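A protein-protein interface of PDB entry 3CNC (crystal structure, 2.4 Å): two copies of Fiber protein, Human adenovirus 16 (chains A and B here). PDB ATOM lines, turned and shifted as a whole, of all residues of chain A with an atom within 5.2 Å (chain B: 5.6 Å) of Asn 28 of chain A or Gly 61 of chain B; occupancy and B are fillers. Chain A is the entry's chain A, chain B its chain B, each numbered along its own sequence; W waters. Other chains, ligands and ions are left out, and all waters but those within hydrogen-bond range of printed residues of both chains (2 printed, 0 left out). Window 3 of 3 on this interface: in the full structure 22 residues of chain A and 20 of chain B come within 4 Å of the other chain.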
ATOM      1  N   GLU A  26       0.697  -4.184 -18.359  1.00  0.00           N
ATOM      2  CA  GLU A  26       1.653  -5.281 -18.464  1.00  0.00           C
ATOM      3  C   GLU A  26       2.812  -5.037 -17.491  1.00  0.00           C
ATOM      4  O   GLU A  26       3.723  -4.259 -17.778  1.00  0.00           O
ATOM      5  CB  GLU A  26       2.173  -5.382 -19.896  1.00  0.00           C
ATOM      6  CG  GLU A  26       1.136  -5.894 -20.875  1.00  0.00           C
ATOM      7  CD  GLU A  26       1.652  -5.931 -22.297  1.00  0.00           C
ATOM      8  OE1 GLU A  26       2.837  -6.291 -22.495  1.00  0.00           O
ATOM      9  OE2 GLU A  26       0.865  -5.613 -23.217  1.00  0.00           O
ATOM     10  N   ASN A  27       2.769  -5.713 -16.343  1.00  0.00           N
ATOM     11  CA  ASN A  27       3.793  -5.557 -15.310  1.00  0.00           C
ATOM     12  C   ASN A  27       5.149  -6.247 -15.563  1.00  0.00           C
ATOM     13  O   ASN A  27       5.992  -6.282 -14.674  1.00  0.00           O
ATOM     14  CB  ASN A  27       3.238  -6.011 -13.961  1.00  0.00           C
ATOM     15  CG  ASN A  27       2.909  -7.488 -13.938  1.00  0.00           C
ATOM     16  OD1 ASN A  27       2.583  -8.040 -12.888  1.00  0.00           O
ATOM     17  ND2 ASN A  27       2.993  -8.139 -15.097  1.00  0.00           N
ATOM     18  N   ASN A  28       5.362  -6.798 -16.755  1.00  0.00           N
ATOM     19  CA  ASN A  28       6.647  -7.432 -17.059  1.00  0.00           C
ATOM     20  C   ASN A  28       7.528  -6.408 -17.778  1.00  0.00           C
ATOM     21  O   ASN A  28       8.616  -6.714 -18.261  1.00  0.00           O
ATOM     22  CB  ASN A  28       6.438  -8.657 -17.946  1.00  0.00           C
ATOM     23  CG  ASN A  28       5.898  -8.299 -19.311  1.00  0.00           C
ATOM     24  OD1 ASN A  28       5.061  -7.409 -19.443  1.00  0.00           O
ATOM     25  ND2 ASN A  28       6.362  -9.000 -20.333  1.00  0.00           N
ATOM     26  N   THR A  29       7.041  -5.177 -17.832  1.00  0.00           N
ATOM     27  CA  THR A  29       7.755  -4.094 -18.490  1.00  0.00           C
ATOM     28  C   THR A  29       7.810  -2.875 -17.592  1.00  0.00           C
ATOM     29  O   THR A  29       6.782  -2.421 -17.085  1.00  0.00           O
ATOM     30  CB  THR A  29       7.058  -3.686 -19.805  1.00  0.00           C
ATOM     31  OG1 THR A  29       7.034  -4.800 -20.702  1.00  0.00           O
ATOM     32  CG2 THR A  29       7.794  -2.538 -20.461  1.00  0.00           C
ATOM     33  N   LEU A  30       9.017  -2.357 -17.387  1.00  0.00           N
ATOM     34  CA  LEU A  30       9.212  -1.159 -16.576  1.00  0.00           C
ATOM     35  C   LEU A  30       9.783  -0.135 -17.560  1.00  0.00           C
ATOM     36  O   LEU A  30      10.851  -0.358 -18.137  1.00  0.00           O
ATOM     37  CB  LEU A  30      10.201  -1.432 -15.437  1.00  0.00           C
ATOM     38  CG  LEU A  30      10.385  -0.288 -14.438  1.00  0.00           C
ATOM     39  CD1 LEU A  30       9.056   0.007 -13.727  1.00  0.00           C
ATOM     40  CD2 LEU A  30      11.453  -0.651 -13.418  1.00  0.00           C
ATOM     41  N   LEU A  57      12.685  -1.482 -19.810  1.00  0.00           N
ATOM     42  CA  LEU A  57      13.293  -2.632 -19.145  1.00  0.00           C
ATOM     43  C   LEU A  57      12.252  -3.752 -19.167  1.00  0.00           C
ATOM     44  O   LEU A  57      11.135  -3.572 -18.680  1.00  0.00           O
ATOM     45  CB  LEU A  57      13.668  -2.278 -17.698  1.00  0.00           C
ATOM     46  CG  LEU A  57      14.663  -1.113 -17.559  1.00  0.00           C
ATOM     47  CD1 LEU A  57      14.955  -0.861 -16.079  1.00  0.00           C
ATOM     48  CD2 LEU A  57      15.933  -1.428 -18.308  1.00  0.00           C
ATOM     49  N   VAL A  58      12.607  -4.896 -19.739  1.00  0.00           N
ATOM     50  CA  VAL A  58      11.667  -6.015 -19.807  1.00  0.00           C
ATOM     51  C   VAL A  58      12.169  -7.322 -19.170  1.00  0.00           C
ATOM     52  O   VAL A  58      13.235  -7.825 -19.529  1.00  0.00           O
ATOM     53  CB  VAL A  58      11.287  -6.330 -21.265  1.00  0.00           C
ATOM     54  CG1 VAL A  58      10.201  -7.393 -21.291  1.00  0.00           C
ATOM     55  CG2 VAL A  58      10.840  -5.061 -21.971  1.00  0.00           C
ATOM     56  N   LYS A  59      11.399  -7.862 -18.230  1.00  0.00           N
ATOM     57  CA  LYS A  59      11.755  -9.121 -17.578  1.00  0.00           C
ATOM     58  C   LYS A  59      11.697 -10.253 -18.590  1.00  0.00           C
ATOM     59  O   LYS A  59      10.646 -10.547 -19.156  1.00  0.00           O
ATOM     60  CB  LYS A  59      10.789  -9.450 -16.445  1.00  0.00           C
ATOM     61  CG  LYS A  59      10.954  -8.632 -15.196  1.00  0.00           C
ATOM     62  CD  LYS A  59       9.994  -9.118 -14.125  1.00  0.00           C
ATOM     63  CE  LYS A  59      10.235  -8.400 -12.814  1.00  0.00           C
ATOM     64  NZ  LYS A  59       9.331  -8.909 -11.747  1.00  0.00           N
ATOM     65  N   LYS A 114       3.830  -0.896 -18.078  1.00  0.00           N
ATOM     66  CA  LYS A 114       3.288  -0.614 -19.386  1.00  0.00           C
ATOM     67  C   LYS A 114       1.770  -0.627 -19.371  1.00  0.00           C
ATOM     68  O   LYS A 114       1.142  -1.586 -18.922  1.00  0.00           O
ATOM     69  CB  LYS A 114       3.790  -1.638 -20.401  1.00  0.00           C
ATOM     70  CG  LYS A 114       3.087  -1.573 -21.736  1.00  0.00           C
ATOM     71  CD  LYS A 114       3.677  -2.581 -22.693  1.00  0.00           C
ATOM     72  CE  LYS A 114       2.804  -2.765 -23.939  1.00  0.00           C
ATOM     73  NZ  LYS A 114       2.748  -1.542 -24.807  1.00  0.00           N
ATOM     74  N   PHE A 130      13.360  -5.809 -11.480  1.00  0.00           N
ATOM     75  CA  PHE A 130      13.885  -5.177 -12.695  1.00  0.00           C
ATOM     76  C   PHE A 130      15.299  -4.647 -12.510  1.00  0.00           C
ATOM     77  O   PHE A 130      15.941  -4.227 -13.473  1.00  0.00           O
ATOM     78  CB  PHE A 130      12.997  -4.001 -13.124  1.00  0.00           C
ATOM     79  CG  PHE A 130      11.653  -4.408 -13.644  1.00  0.00           C
ATOM     80  CD1 PHE A 130      10.551  -4.465 -12.798  1.00  0.00           C
ATOM     81  CD2 PHE A 130      11.489  -4.743 -14.988  1.00  0.00           C
ATOM     82  CE1 PHE A 130       9.284  -4.857 -13.291  1.00  0.00           C
ATOM     83  CE2 PHE A 130      10.247  -5.131 -15.492  1.00  0.00           C
ATOM     84  CZ  PHE A 130       9.140  -5.189 -14.644  1.00  0.00           C
ATOM     85  N   LYS B  59       7.184 -11.117 -29.308  1.00  0.00           N
ATOM     86  CA  LYS B  59       6.627 -10.172 -28.350  1.00  0.00           C
ATOM     87  C   LYS B  59       7.297 -10.424 -27.008  1.00  0.00           C
ATOM     88  O   LYS B  59       7.182 -11.517 -26.450  1.00  0.00           O
ATOM     89  CB  LYS B  59       5.122 -10.373 -28.175  1.00  0.00           C
ATOM     90  CG  LYS B  59       4.267  -9.892 -29.322  1.00  0.00           C
ATOM     91  CD  LYS B  59       2.805 -10.070 -28.980  1.00  0.00           C
ATOM     92  CE  LYS B  59       1.917  -9.667 -30.133  1.00  0.00           C
ATOM     93  NZ  LYS B  59       0.476  -9.868 -29.803  1.00  0.00           N
ATOM     94  N   ASN B  60       7.973  -9.408 -26.485  1.00  0.00           N
ATOM     95  CA  ASN B  60       8.681  -9.511 -25.213  1.00  0.00           C
ATOM     96  C   ASN B  60       8.351  -8.250 -24.423  1.00  0.00           C
ATOM     97  O   ASN B  60       9.114  -7.288 -24.417  1.00  0.00           O
ATOM     98  CB  ASN B  60      10.189  -9.634 -25.500  1.00  0.00           C
ATOM     99  CG  ASN B  60      11.024  -9.907 -24.251  1.00  0.00           C
ATOM    100  OD1 ASN B  60      10.600 -10.617 -23.330  1.00  0.00           O
ATOM    101  ND2 ASN B  60      12.231  -9.361 -24.232  1.00  0.00           N
ATOM    102  N   GLY B  61       7.195  -8.271 -23.763  1.00  0.00           N
ATOM    103  CA  GLY B  61       6.748  -7.126 -22.994  1.00  0.00           C
ATOM    104  C   GLY B  61       6.393  -5.990 -23.942  1.00  0.00           C
ATOM    105  O   GLY B  61       5.750  -6.219 -24.965  1.00  0.00           O
ATOM    106  N   GLY B  62       6.819  -4.771 -23.619  1.00  0.00           N
ATOM    107  CA  GLY B  62       6.535  -3.638 -24.485  1.00  0.00           C
ATOM    108  C   GLY B  62       7.433  -3.602 -25.715  1.00  0.00           C
ATOM    109  O   GLY B  62       7.310  -2.719 -26.565  1.00  0.00           O
ATOM    110  N   LEU B  63       8.344  -4.561 -25.818  1.00  0.00           N
ATOM    111  CA  LEU B  63       9.253  -4.609 -26.953  1.00  0.00           C
ATOM    112  C   LEU B  63       8.993  -5.799 -27.851  1.00  0.00           C
ATOM    113  O   LEU B  63       8.220  -6.695 -27.528  1.00  0.00           O
ATOM    114  CB  LEU B  63      10.712  -4.705 -26.486  1.00  0.00           C
ATOM    115  CG  LEU B  63      11.309  -3.605 -25.605  1.00  0.00           C
ATOM    116  CD1 LEU B  63      12.717  -4.009 -25.163  1.00  0.00           C
ATOM    117  CD2 LEU B  63      11.340  -2.280 -26.381  1.00  0.00           C
ATOM    118  N   ARG B 217       6.787  -1.721 -29.332  1.00  0.00           N
ATOM    119  CA  ARG B 217       5.725  -2.279 -30.146  1.00  0.00           C
ATOM    120  C   ARG B 217       4.362  -1.635 -30.026  1.00  0.00           C
ATOM    121  O   ARG B 217       3.991  -1.068 -28.988  1.00  0.00           O
ATOM    122  CB  ARG B 217       5.594  -3.792 -29.878  1.00  0.00           C
ATOM    123  CG  ARG B 217       4.817  -4.144 -28.628  1.00  0.00           C
ATOM    124  CD  ARG B 217       4.947  -5.623 -28.275  1.00  0.00           C
ATOM    125  NE  ARG B 217       4.086  -5.958 -27.146  1.00  0.00           N
ATOM    126  CZ  ARG B 217       2.785  -6.188 -27.256  1.00  0.00           C
ATOM    127  NH1 ARG B 217       2.204  -6.131 -28.446  1.00  0.00           N
ATOM    128  NH2 ARG B 217       2.058  -6.449 -26.180  1.00  0.00           N
HETATM  129  O   HOH W   1      -1.015  -4.924 -25.973  1.00  0.00           O
HETATM  130  O   HOH W   2       4.846  -1.074 -26.298  1.00  0.00           O
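The side-chain carboxylate (OE2) of Glu 26 of chain A lies within salt-bridge range of the guanidinium group (NH2) of Arg 217 of chain B, at 3.3 Å. The side-chain hydroxyl of Thr 29 of chain A is in hydrogen-bond range of the backbone NH of Gly 62 of chain B (2.9 Å).
N of Glu 26 of chain A sits at hydrogen-bond distance from O of Lys 114 of chain A (2.7 Å). O of Gly 62 of chain B sits at hydrogen-bond distance from N of Arg 217 of chain B (3.0 Å). The backbone carbonyl oxygen of Asn 28 of chain A sits at hydrogen-bond distance from the backbone NH of Lys 59 of chain A, at 3.0 Å. The backbone carbonyl oxygen (O) of Gly 61 of chain B is in hydrogen-bond range of the guanidinium group (NE) of Arg 217 of chain B (2.8 Å). The backbone NH of Lys 114 of chain A sits at hydrogen-bond distance from the backbone carbonyl oxygen of Thr 29 of chain A (3.5 Å).
Among the printed residues, pairs that only touch across the chains: Glu 26 of chain A with Gly 61 of chain B, Asn 28 of chain A with Gly 61 of chain B, Thr 29 of chain A with Gly 61 of chain B, Val 58 of chain A with Asn 60 of chain B, Val 58 of chain A with Gly 61 of chain B, Val 58 of chain A with Leu 63 of chain B and Lys 114 of chain A with Gly 62 of chain B.
Of the printed residues of chain B, Glu 26 of chain A touches Gly 61 (3.8 Å) and Arg 217 (3.3 Å). Of the printed residues of chain B, Thr 29 of chain A touches Gly 61 (3.3 Å) and Gly 62 (2.9 Å). Leu 57 of chain A touches none of the printed residues of chain B. Printed residues of chain A within 4 Å of Asn 60 of chain B: Val 58 (3.3 Å). Gly 61 of chain B touches just these residues of chain A: Glu 26, Asn 28, Thr 29 and Val 58. Of the printed residues of chain A, Arg 217 of chain B touches Glu 26 (3.3 Å). The nearest residue of chain B that does not touch Asn 28 of chain A is Asn 60 of chain B (4.6 Å). The nearest residue of chain A that does not touch Gly 61 of chain B is Lys 114 of chain A (4.5 Å).
Hydrophobic or aromatic side chains of chain A within 4 Å of the printed part of chain B: Val 58.
Position printed for both chains: 59.
Water W2 lies within hydrogen-bond range of the side-chain amino group of Lys 114 of chain A, the backbone carbonyl oxygen of Arg 217 of chain B and the backbone carbonyl oxygen of Gly 62 of chain B. Water W1 bridges OE2 of Glu 26 of chain A (3.4 Å) and NH2 of Arg 217 of chain B (3.4 Å).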
